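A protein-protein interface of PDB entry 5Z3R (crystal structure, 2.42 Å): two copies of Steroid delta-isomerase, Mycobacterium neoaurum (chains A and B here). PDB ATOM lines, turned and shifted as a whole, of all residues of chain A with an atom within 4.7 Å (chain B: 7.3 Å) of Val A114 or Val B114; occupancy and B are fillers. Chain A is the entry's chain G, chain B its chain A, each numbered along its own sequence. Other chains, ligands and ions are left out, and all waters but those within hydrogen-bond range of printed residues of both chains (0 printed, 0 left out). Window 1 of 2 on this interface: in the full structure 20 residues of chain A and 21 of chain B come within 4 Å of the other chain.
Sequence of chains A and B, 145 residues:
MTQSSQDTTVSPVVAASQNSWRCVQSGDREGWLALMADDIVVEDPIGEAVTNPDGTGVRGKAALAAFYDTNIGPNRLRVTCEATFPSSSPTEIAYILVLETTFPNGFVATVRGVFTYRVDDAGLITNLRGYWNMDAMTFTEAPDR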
ATOM      1  N   PHE A  85     -16.246 -18.846 -13.786  1.00  0.00           N
ATOM      2  CA  PHE A  85     -15.102 -19.728 -14.022  1.00  0.00           C
ATOM      3  C   PHE A  85     -14.872 -20.559 -12.760  1.00  0.00           C
ATOM      4  O   PHE A  85     -14.049 -20.162 -11.903  1.00  0.00           O
ATOM      5  CB  PHE A  85     -13.850 -18.926 -14.357  1.00  0.00           C
ATOM      6  CG  PHE A  85     -13.990 -18.081 -15.570  1.00  0.00           C
ATOM      7  CD1 PHE A  85     -14.467 -16.777 -15.472  1.00  0.00           C
ATOM      8  CD2 PHE A  85     -13.641 -18.571 -16.814  1.00  0.00           C
ATOM      9  CE1 PHE A  85     -14.625 -15.980 -16.610  1.00  0.00           C
ATOM     10  CE2 PHE A  85     -13.803 -17.791 -17.960  1.00  0.00           C
ATOM     11  CZ  PHE A  85     -14.283 -16.484 -17.858  1.00  0.00           C
ATOM     12  N   ALA A  94     -14.078 -17.899  -9.496  1.00  0.00           N
ATOM     13  CA  ALA A  94     -13.770 -16.581 -10.061  1.00  0.00           C
ATOM     14  C   ALA A  94     -14.890 -16.199 -10.988  1.00  0.00           C
ATOM     15  O   ALA A  94     -15.361 -17.046 -11.750  1.00  0.00           O
ATOM     16  CB  ALA A  94     -12.452 -16.617 -10.842  1.00  0.00           C
ATOM     17  N   TYR A  95     -15.278 -14.924 -10.944  1.00  0.00           N
ATOM     18  CA  TYR A  95     -16.254 -14.352 -11.861  1.00  0.00           C
ATOM     19  C   TYR A  95     -15.704 -13.150 -12.646  1.00  0.00           C
ATOM     20  O   TYR A  95     -14.735 -12.551 -12.247  1.00  0.00           O
ATOM     21  CB  TYR A  95     -17.415 -13.837 -11.050  1.00  0.00           C
ATOM     22  CG  TYR A  95     -18.166 -14.850 -10.240  1.00  0.00           C
ATOM     23  CD1 TYR A  95     -19.113 -15.665 -10.845  1.00  0.00           C
ATOM     24  CD2 TYR A  95     -17.999 -14.936  -8.874  1.00  0.00           C
ATOM     25  CE1 TYR A  95     -19.852 -16.562 -10.122  1.00  0.00           C
ATOM     26  CE2 TYR A  95     -18.741 -15.823  -8.131  1.00  0.00           C
ATOM     27  CZ  TYR A  95     -19.680 -16.641  -8.770  1.00  0.00           C
ATOM     28  OH  TYR A  95     -20.449 -17.559  -8.073  1.00  0.00           O
ATOM     29  N   ILE A  96     -16.361 -12.812 -13.755  1.00  0.00           N
ATOM     30  CA  ILE A  96     -16.328 -11.478 -14.309  1.00  0.00           C
ATOM     31  C   ILE A  96     -17.608 -10.801 -13.876  1.00  0.00           C
ATOM     32  O   ILE A  96     -18.688 -11.223 -14.282  1.00  0.00           O
ATOM     33  CB  ILE A  96     -16.209 -11.492 -15.856  1.00  0.00           C
ATOM     34  CG1 ILE A  96     -14.811 -11.959 -16.238  1.00  0.00           C
ATOM     35  CG2 ILE A  96     -16.394 -10.112 -16.481  1.00  0.00           C
ATOM     36  CD1 ILE A  96     -14.532 -11.893 -17.736  1.00  0.00           C
ATOM     37  N   GLY A 113     -14.517  -6.069 -13.688  1.00  0.00           N
ATOM     38  CA  GLY A 113     -13.299  -6.688 -13.202  1.00  0.00           C
ATOM     39  C   GLY A 113     -13.512  -8.164 -12.899  1.00  0.00           C
ATOM     40  O   GLY A 113     -14.641  -8.668 -12.960  1.00  0.00           O
ATOM     41  N   VAL A 114     -12.412  -8.842 -12.574  1.00  0.00           N
ATOM     42  CA  VAL A 114     -12.464 -10.203 -12.151  1.00  0.00           C
ATOM     43  C   VAL A 114     -12.610 -10.196 -10.637  1.00  0.00           C
ATOM     44  O   VAL A 114     -11.862  -9.510  -9.972  1.00  0.00           O
ATOM     45  CB  VAL A 114     -11.214 -10.990 -12.586  1.00  0.00           C
ATOM     46  CG1 VAL A 114     -11.056 -12.269 -11.796  1.00  0.00           C
ATOM     47  CG2 VAL A 114     -11.273 -11.307 -14.074  1.00  0.00           C
ATOM     48  N   PHE A 115     -13.534 -11.016 -10.119  1.00  0.00           N
ATOM     49  CA  PHE A 115     -13.776 -11.176  -8.691  1.00  0.00           C
ATOM     50  C   PHE A 115     -13.611 -12.620  -8.297  1.00  0.00           C
ATOM     51  O   PHE A 115     -14.321 -13.469  -8.813  1.00  0.00           O
ATOM     52  CB  PHE A 115     -15.185 -10.703  -8.339  1.00  0.00           C
ATOM     53  CG  PHE A 115     -15.337  -9.226  -8.452  1.00  0.00           C
ATOM     54  CD1 PHE A 115     -15.536  -8.644  -9.673  1.00  0.00           C
ATOM     55  CD2 PHE A 115     -15.191  -8.419  -7.340  1.00  0.00           C
ATOM     56  CE1 PHE A 115     -15.631  -7.260  -9.796  1.00  0.00           C
ATOM     57  CE2 PHE A 115     -15.301  -7.036  -7.439  1.00  0.00           C
ATOM     58  CZ  PHE A 115     -15.505  -6.448  -8.666  1.00  0.00           C
ATOM     59  N   THR A 116     -12.654 -12.897  -7.422  1.00  0.00           N
ATOM     60  CA  THR A 116     -12.479 -14.212  -6.890  1.00  0.00           C
ATOM     61  C   THR A 116     -13.042 -14.276  -5.471  1.00  0.00           C
ATOM     62  O   THR A 116     -12.902 -13.303  -4.707  1.00  0.00           O
ATOM     63  CB  THR A 116     -11.006 -14.633  -6.817  1.00  0.00           C
ATOM     64  OG1 THR A 116     -10.309 -13.786  -5.909  1.00  0.00           O
ATOM     65  CG2 THR A 116     -10.382 -14.601  -8.145  1.00  0.00           C
ATOM     66  N   ARG A 129     -11.937 -10.723  -3.457  1.00  0.00           N
ATOM     67  CA  ARG A 129     -10.799 -10.022  -4.074  1.00  0.00           C
ATOM     68  C   ARG A 129     -11.203  -9.552  -5.479  1.00  0.00           C
ATOM     69  O   ARG A 129     -11.771 -10.339  -6.239  1.00  0.00           O
ATOM     70  CB  ARG A 129      -9.592 -10.971  -4.133  1.00  0.00           C
ATOM     71  CG  ARG A 129      -8.825 -11.038  -2.824  1.00  0.00           C
ATOM     72  CD  ARG A 129      -7.926 -12.242  -2.627  1.00  0.00           C
ATOM     73  NE  ARG A 129      -6.838 -12.323  -3.595  1.00  0.00           N
ATOM     74  CZ  ARG A 129      -5.710 -11.601  -3.619  1.00  0.00           C
ATOM     75  NH1 ARG A 129      -5.449 -10.688  -2.731  1.00  0.00           N
ATOM     76  NH2 ARG A 129      -4.837 -11.793  -4.592  1.00  0.00           N
ATOM     77  N   GLY A 130     -10.948  -8.271  -5.808  1.00  0.00           N
ATOM     78  CA  GLY A 130     -11.390  -7.644  -7.064  1.00  0.00           C
ATOM     79  C   GLY A 130     -10.202  -7.149  -7.871  1.00  0.00           C
ATOM     80  O   GLY A 130      -9.402  -6.359  -7.375  1.00  0.00           O
ATOM     81  N   TYR A 131     -10.080  -7.634  -9.109  1.00  0.00           N
ATOM     82  CA  TYR A 131      -9.013  -7.247 -10.033  1.00  0.00           C
ATOM     83  C   TYR A 131      -9.592  -6.138 -10.939  1.00  0.00           C
ATOM     84  O   TYR A 131     -10.187  -6.390 -11.964  1.00  0.00           O
ATOM     85  CB  TYR A 131      -8.542  -8.423 -10.883  1.00  0.00           C
ATOM     86  CG  TYR A 131      -7.834  -9.440 -10.112  1.00  0.00           C
ATOM     87  CD1 TYR A 131      -8.536 -10.306  -9.270  1.00  0.00           C
ATOM     88  CD2 TYR A 131      -6.459  -9.546 -10.175  1.00  0.00           C
ATOM     89  CE1 TYR A 131      -7.872 -11.243  -8.498  1.00  0.00           C
ATOM     90  CE2 TYR A 131      -5.777 -10.494  -9.422  1.00  0.00           C
ATOM     91  CZ  TYR A 131      -6.462 -11.338  -8.568  1.00  0.00           C
ATOM     92  OH  TYR A 131      -5.784 -12.296  -7.787  1.00  0.00           O
ATOM     93  N   ILE B  46      -6.735 -24.724  -9.461  1.00  0.00           N
ATOM     94  CA  ILE B  46      -7.019 -24.792  -8.045  1.00  0.00           C
ATOM     95  C   ILE B  46      -7.930 -25.995  -7.821  1.00  0.00           C
ATOM     96  O   ILE B  46      -8.926 -26.197  -8.547  1.00  0.00           O
ATOM     97  CB  ILE B  46      -7.751 -23.504  -7.541  1.00  0.00           C
ATOM     98  CG1 ILE B  46      -6.865 -22.247  -7.739  1.00  0.00           C
ATOM     99  CG2 ILE B  46      -8.177 -23.662  -6.071  1.00  0.00           C
ATOM    100  CD1 ILE B  46      -7.605 -20.906  -7.717  1.00  0.00           C
ATOM    101  N   ALA B  83      -8.033 -11.473 -22.454  1.00  0.00           N
ATOM    102  CA  ALA B  83      -8.347 -10.302 -21.647  1.00  0.00           C
ATOM    103  C   ALA B  83      -7.412 -10.165 -20.449  1.00  0.00           C
ATOM    104  O   ALA B  83      -7.018 -11.169 -19.866  1.00  0.00           O
ATOM    105  CB  ALA B  83      -9.775 -10.359 -21.147  1.00  0.00           C
ATOM    106  N   THR B  84      -7.099  -8.909 -20.090  1.00  0.00           N
ATOM    107  CA  THR B  84      -6.240  -8.558 -18.977  1.00  0.00           C
ATOM    108  C   THR B  84      -7.112  -7.857 -17.976  1.00  0.00           C
ATOM    109  O   THR B  84      -7.932  -7.041 -18.335  1.00  0.00           O
ATOM    110  CB  THR B  84      -5.011  -7.679 -19.416  1.00  0.00           C
ATOM    111  OG1 THR B  84      -5.408  -6.329 -19.770  1.00  0.00           O
ATOM    112  CG2 THR B  84      -4.305  -8.294 -20.667  1.00  0.00           C
ATOM    113  N   PHE B  85      -6.974  -8.196 -16.702  1.00  0.00           N
ATOM    114  CA  PHE B  85      -7.671  -7.477 -15.661  1.00  0.00           C
ATOM    115  C   PHE B  85      -6.638  -7.051 -14.630  1.00  0.00           C
ATOM    116  O   PHE B  85      -6.510  -7.708 -13.598  1.00  0.00           O
ATOM    117  CB  PHE B  85      -8.742  -8.369 -15.022  1.00  0.00           C
ATOM    118  CG  PHE B  85      -9.865  -8.666 -15.951  1.00  0.00           C
ATOM    119  CD1 PHE B  85     -10.915  -7.772 -16.087  1.00  0.00           C
ATOM    120  CD2 PHE B  85      -9.850  -9.808 -16.748  1.00  0.00           C
ATOM    121  CE1 PHE B  85     -11.951  -8.018 -16.988  1.00  0.00           C
ATOM    122  CE2 PHE B  85     -10.871 -10.051 -17.645  1.00  0.00           C
ATOM    123  CZ  PHE B  85     -11.921  -9.158 -17.770  1.00  0.00           C
ATOM    124  N   PRO B  86      -5.904  -5.950 -14.898  1.00  0.00           N
ATOM    125  CA  PRO B  86      -5.038  -5.395 -13.838  1.00  0.00           C
ATOM    126  C   PRO B  86      -5.824  -4.967 -12.628  1.00  0.00           C
ATOM    127  O   PRO B  86      -6.990  -4.578 -12.738  1.00  0.00           O
ATOM    128  CB  PRO B  86      -4.353  -4.172 -14.496  1.00  0.00           C
ATOM    129  CG  PRO B  86      -5.095  -3.927 -15.794  1.00  0.00           C
ATOM    130  CD  PRO B  86      -5.785  -5.219 -16.182  1.00  0.00           C
ATOM    131  N   ILE B  93      -2.345  -9.517 -10.837  1.00  0.00           N
ATOM    132  CA  ILE B  93      -3.182  -9.336 -12.033  1.00  0.00           C
ATOM    133  C   ILE B  93      -3.982 -10.622 -12.327  1.00  0.00           C
ATOM    134  O   ILE B  93      -3.613 -11.682 -11.891  1.00  0.00           O
ATOM    135  CB  ILE B  93      -2.301  -8.955 -13.214  1.00  0.00           C
ATOM    136  CG1 ILE B  93      -3.157  -8.595 -14.446  1.00  0.00           C
ATOM    137  CG2 ILE B  93      -1.305 -10.085 -13.483  1.00  0.00           C
ATOM    138  CD1 ILE B  93      -2.465  -7.700 -15.484  1.00  0.00           C
ATOM    139  N   ALA B  94      -5.066 -10.500 -13.068  1.00  0.00           N
ATOM    140  CA  ALA B  94      -5.851 -11.642 -13.533  1.00  0.00           C
ATOM    141  C   ALA B  94      -5.968 -11.574 -15.021  1.00  0.00           C
ATOM    142  O   ALA B  94      -5.886 -10.498 -15.646  1.00  0.00           O
ATOM    143  CB  ALA B  94      -7.231 -11.644 -12.904  1.00  0.00           C
ATOM    144  N   TYR B  95      -6.055 -12.752 -15.612  1.00  0.00           N
ATOM    145  CA  TYR B  95      -6.218 -12.837 -17.054  1.00  0.00           C
ATOM    146  C   TYR B  95      -7.269 -13.865 -17.382  1.00  0.00           C
ATOM    147  O   TYR B  95      -7.649 -14.651 -16.548  1.00  0.00           O
ATOM    148  CB  TYR B  95      -4.954 -13.266 -17.707  1.00  0.00           C
ATOM    149  CG  TYR B  95      -3.733 -12.411 -17.583  1.00  0.00           C
ATOM    150  CD1 TYR B  95      -3.497 -11.375 -18.482  1.00  0.00           C
ATOM    151  CD2 TYR B  95      -2.719 -12.726 -16.663  1.00  0.00           C
ATOM    152  CE1 TYR B  95      -2.325 -10.671 -18.448  1.00  0.00           C
ATOM    153  CE2 TYR B  95      -1.535 -12.004 -16.626  1.00  0.00           C
ATOM    154  CZ  TYR B  95      -1.341 -10.972 -17.521  1.00  0.00           C
ATOM    155  OH  TYR B  95      -0.165 -10.235 -17.522  1.00  0.00           O
ATOM    156  N   ILE B  96      -7.732 -13.825 -18.611  1.00  0.00           N
ATOM    157  CA  ILE B  96      -8.487 -14.900 -19.221  1.00  0.00           C
ATOM    158  C   ILE B  96      -7.472 -15.420 -20.207  1.00  0.00           C
ATOM    159  O   ILE B  96      -7.100 -14.719 -21.192  1.00  0.00           O
ATOM    160  CB  ILE B  96      -9.742 -14.439 -19.978  1.00  0.00           C
ATOM    161  CG1 ILE B  96     -10.636 -13.588 -19.078  1.00  0.00           C
ATOM    162  CG2 ILE B  96     -10.500 -15.615 -20.558  1.00  0.00           C
ATOM    163  CD1 ILE B  96     -11.351 -14.321 -17.978  1.00  0.00           C
ATOM    164  N   LEU B  97      -6.983 -16.621 -19.917  1.00  0.00           N
ATOM    165  CA  LEU B  97      -6.171 -17.350 -20.860  1.00  0.00           C
ATOM    166  C   LEU B  97      -6.889 -18.587 -21.398  1.00  0.00           C
ATOM    167  O   LEU B  97      -7.744 -19.182 -20.730  1.00  0.00           O
ATOM    168  CB  LEU B  97      -4.881 -17.784 -20.192  1.00  0.00           C
ATOM    169  CG  LEU B  97      -4.153 -16.788 -19.317  1.00  0.00           C
ATOM    170  CD1 LEU B  97      -2.873 -17.448 -18.841  1.00  0.00           C
ATOM    171  CD2 LEU B  97      -3.836 -15.588 -20.186  1.00  0.00           C
ATOM    172  N   ARG B 112     -10.097 -22.982 -21.222  1.00  0.00           N
ATOM    173  CA  ARG B 112     -10.263 -21.562 -20.998  1.00  0.00           C
ATOM    174  C   ARG B 112     -10.487 -21.404 -19.499  1.00  0.00           C
ATOM    175  O   ARG B 112     -11.255 -22.175 -18.888  1.00  0.00           O
ATOM    176  CB  ARG B 112     -11.430 -21.027 -21.797  1.00  0.00           C
ATOM    177  CG  ARG B 112     -11.504 -19.499 -21.919  1.00  0.00           C
ATOM    178  CD  ARG B 112     -12.382 -19.104 -23.123  1.00  0.00           C
ATOM    179  NE  ARG B 112     -12.876 -17.730 -23.052  1.00  0.00           N
ATOM    180  CZ  ARG B 112     -13.830 -17.270 -22.224  1.00  0.00           C
ATOM    181  NH1 ARG B 112     -14.439 -18.074 -21.348  1.00  0.00           N
ATOM    182  NH2 ARG B 112     -14.173 -15.964 -22.246  1.00  0.00           N
ATOM    183  N   GLY B 113      -9.770 -20.446 -18.899  1.00  0.00           N
ATOM    184  CA  GLY B 113      -9.901 -20.139 -17.469  1.00  0.00           C
ATOM    185  C   GLY B 113      -9.424 -18.738 -17.089  1.00  0.00           C
ATOM    186  O   GLY B 113      -8.814 -18.021 -17.904  1.00  0.00           O
ATOM    187  N   VAL B 114      -9.785 -18.328 -15.873  1.00  0.00           N
ATOM    188  CA  VAL B 114      -9.171 -17.202 -15.232  1.00  0.00           C
ATOM    189  C   VAL B 114      -7.886 -17.596 -14.526  1.00  0.00           C
ATOM    190  O   VAL B 114      -7.894 -18.496 -13.733  1.00  0.00           O
ATOM    191  CB  VAL B 114     -10.087 -16.538 -14.232  1.00  0.00           C
ATOM    192  CG1 VAL B 114      -9.311 -15.481 -13.406  1.00  0.00           C
ATOM    193  CG2 VAL B 114     -11.242 -15.889 -14.972  1.00  0.00           C
ATOM    194  N   PHE B 115      -6.808 -16.854 -14.784  1.00  0.00           N
ATOM    195  CA  PHE B 115      -5.493 -17.101 -14.208  1.00  0.00           C
ATOM    196  C   PHE B 115      -5.027 -15.859 -13.487  1.00  0.00           C
ATOM    197  O   PHE B 115      -4.877 -14.789 -14.098  1.00  0.00           O
ATOM    198  CB  PHE B 115      -4.491 -17.478 -15.295  1.00  0.00           C
ATOM    199  CG  PHE B 115      -4.748 -18.810 -15.882  1.00  0.00           C
ATOM    200  CD1 PHE B 115      -5.796 -18.995 -16.771  1.00  0.00           C
ATOM    201  CD2 PHE B 115      -3.979 -19.896 -15.528  1.00  0.00           C
ATOM    202  CE1 PHE B 115      -6.068 -20.242 -17.317  1.00  0.00           C
ATOM    203  CE2 PHE B 115      -4.247 -21.146 -16.056  1.00  0.00           C
ATOM    204  CZ  PHE B 115      -5.286 -21.316 -16.960  1.00  0.00           C
ATOM    205  N   THR B 116      -4.816 -16.008 -12.185  1.00  0.00           N
ATOM    206  CA  THR B 116      -4.299 -14.951 -11.364  1.00  0.00           C
ATOM    207  C   THR B 116      -2.817 -15.124 -11.109  1.00  0.00           C
ATOM    208  O   THR B 116      -2.365 -16.233 -10.849  1.00  0.00           O
ATOM    209  CB  THR B 116      -4.981 -14.856  -9.989  1.00  0.00           C
ATOM    210  OG1 THR B 116      -4.617 -15.976  -9.206  1.00  0.00           O
ATOM    211  CG2 THR B 116      -6.514 -14.694 -10.107  1.00  0.00           C
ATOM    212  N   LEU B 128       0.622 -18.681  -8.868  1.00  0.00           N
ATOM    213  CA  LEU B 128      -0.018 -18.792 -10.186  1.00  0.00           C
ATOM    214  C   LEU B 128      -1.202 -19.694  -9.943  1.00  0.00           C
ATOM    215  O   LEU B 128      -1.040 -20.785  -9.427  1.00  0.00           O
ATOM    216  CB  LEU B 128       0.898 -19.372 -11.242  1.00  0.00           C
ATOM    217  CG  LEU B 128       0.525 -19.129 -12.717  1.00  0.00           C
ATOM    218  CD1 LEU B 128       1.450 -19.870 -13.670  1.00  0.00           C
ATOM    219  CD2 LEU B 128      -0.924 -19.482 -13.035  1.00  0.00           C
ATOM    220  N   ARG B 129      -2.393 -19.200 -10.247  1.00  0.00           N
ATOM    221  CA  ARG B 129      -3.633 -19.829  -9.823  1.00  0.00           C
ATOM    222  C   ARG B 129      -4.615 -19.860 -10.984  1.00  0.00           C
ATOM    223  O   ARG B 129      -4.855 -18.845 -11.578  1.00  0.00           O
ATOM    224  CB  ARG B 129      -4.177 -19.120  -8.586  1.00  0.00           C
ATOM    225  CG  ARG B 129      -3.306 -19.456  -7.375  1.00  0.00           C
ATOM    226  CD  ARG B 129      -3.656 -18.677  -6.149  1.00  0.00           C
ATOM    227  NE  ARG B 129      -5.007 -18.996  -5.738  1.00  0.00           N
ATOM    228  CZ  ARG B 129      -5.357 -19.951  -4.887  1.00  0.00           C
ATOM    229  NH1 ARG B 129      -4.464 -20.727  -4.311  1.00  0.00           N
ATOM    230  NH2 ARG B 129      -6.621 -20.121  -4.585  1.00  0.00           N
ATOM    231  N   GLY B 130      -5.101 -21.058 -11.334  1.00  0.00           N
ATOM    232  CA  GLY B 130      -5.976 -21.291 -12.501  1.00  0.00           C
ATOM    233  C   GLY B 130      -7.377 -21.679 -12.053  1.00  0.00           C
ATOM    234  O   GLY B 130      -7.557 -22.609 -11.262  1.00  0.00           O
ATOM    235  N   TYR B 131      -8.358 -20.928 -12.530  1.00  0.00           N
ATOM    236  CA  TYR B 131      -9.756 -21.216 -12.277  1.00  0.00           C
ATOM    237  C   TYR B 131     -10.352 -21.936 -13.507  1.00  0.00           C
ATOM    238  O   TYR B 131     -10.807 -21.279 -14.466  1.00  0.00           O
ATOM    239  CB  TYR B 131     -10.542 -19.940 -11.948  1.00  0.00           C
ATOM    240  CG  TYR B 131     -10.202 -19.278 -10.644  1.00  0.00           C
ATOM    241  CD1 TYR B 131      -9.066 -18.481 -10.521  1.00  0.00           C
ATOM    242  CD2 TYR B 131     -11.023 -19.413  -9.530  1.00  0.00           C
ATOM    243  CE1 TYR B 131      -8.733 -17.883  -9.311  1.00  0.00           C
ATOM    244  CE2 TYR B 131     -10.699 -18.802  -8.323  1.00  0.00           C
ATOM    245  CZ  TYR B 131      -9.543 -18.037  -8.231  1.00  0.00           C
ATOM    246  OH  TYR B 131      -9.211 -17.412  -7.081  1.00  0.00           O
ATOM    247  N   TRP B 132     -10.326 -23.277 -13.444  1.00  0.00           N
ATOM    248  CA  TRP B 132     -10.926 -24.197 -14.420  1.00  0.00           C
ATOM    249  C   TRP B 132     -11.062 -25.639 -13.880  1.00  0.00           C
ATOM    250  O   TRP B 132     -10.396 -26.019 -12.904  1.00  0.00           O
ATOM    251  CB  TRP B 132     -10.091 -24.241 -15.692  1.00  0.00           C
ATOM    252  CG  TRP B 132      -8.646 -24.722 -15.575  1.00  0.00           C
ATOM    253  CD1 TRP B 132      -7.557 -23.942 -15.421  1.00  0.00           C
ATOM    254  CD2 TRP B 132      -8.149 -26.058 -15.723  1.00  0.00           C
ATOM    255  NE1 TRP B 132      -6.413 -24.693 -15.416  1.00  0.00           N
ATOM    256  CE2 TRP B 132      -6.742 -25.997 -15.608  1.00  0.00           C
ATOM    257  CE3 TRP B 132      -8.749 -27.307 -15.913  1.00  0.00           C
ATOM    258  CZ2 TRP B 132      -5.912 -27.142 -15.693  1.00  0.00           C
ATOM    259  CZ3 TRP B 132      -7.905 -28.473 -15.994  1.00  0.00           C
ATOM    260  CH2 TRP B 132      -6.514 -28.366 -15.888  1.00  0.00           C
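Printed residues of chain B that touch a printed residue of chain A: Phe B85, Pro B86, Ile B93, Ala B94, Ile B96, Arg B112, Val B114, Thr B116 and Tyr B131.
Hydrophobic or aromatic side chains of chain B within 4 Å of the printed part of chain A: Phe B85, Ala B94, Ile B96, Val B114 and Tyr B131.
Along chain B the printed residues that touch a printed residue of chain A span positions 85 to 131.
Hydrophobic or aromatic side chains of chain A that line the printed part of chain B: Phe A85, Ala A94, Ile A96, Val A114 and Tyr A131.
Among the printed residues, 15 pairs touch across the chains.
Among the printed residues, no Asp or Glu carboxylate lies within 4 Å of a Lys or Arg side-chain nitrogen of the other chain.
Among the printed residues, pairs that only touch across the chains: Thr A116 with Tyr B131, Tyr A131 with Ala B94, Val A114 with Phe B85, Phe A85 with Val B114, Ala A94 with Tyr B131, Tyr A131 with Thr B116, Tyr A131 with Ile B93, Phe A85 with Arg B112, Tyr A131 with Phe B85, Phe A85 with Tyr B131, Tyr A131 with Pro B86, Phe A85 with Ile B96, Ile A96 with Phe B85, Gly A113 with Phe B85 and Val A114 with Val B114.
Of the printed residues of chain B, Ile A96 touches Phe B85.
Of the printed residues of chain B, Val A114 touches Phe B85 and Val B114.
Gly A130 touches none of the printed residues of chain B.
Printed residues of chain A within 4 Å of Phe B85: Ile A96 (3.8 Å), Gly A113 (3.9 Å), Val A114 (3.4 Å) and Tyr A131 (3.5 Å).
Of the printed residues of chain A, Val B114 touches Phe A85 and Val A114.
The backbone NH (N) of Thr B116 sits at hydrogen-bond distance from the backbone carbonyl oxygen (O) of Arg B129, 2.9 Å away.
The backbone carbonyl oxygen (O) of Val A114 is in hydrogen-bond range of the backbone NH (N) of Tyr A131 (2.7 Å).
N of Tyr B131 sits at hydrogen-bond distance from O of Val B114 (2.8 Å).
The backbone carbonyl oxygen (O) of Ala B94 is in hydrogen-bond range of the backbone NH (N) of Phe B85, at 2.8 Å.
OH of Tyr A131 sits at hydrogen-bond distance from NH2 of Arg A129, at 3.4 Å.
The backbone carbonyl oxygen of Arg A129 is in hydrogen-bond range of the backbone NH of Thr A116 (3.0 Å).
Phe A85 touches Ile B96, and with the chains exchanged Ile A96 touches Phe B85.
Phe A85 touches Tyr B131, and with the chains exchanged Tyr A131 touches Phe B85.
Gly A113 touches Phe B85, but with the chains exchanged Phe A85 does not touch Gly B113 (4.1 Å).
Val B114 touches its own counterpart, Val A114.
Of the 15 pairs that touch across the chains among the printed residues, 11 have their exchanged pair printed and touching as well.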
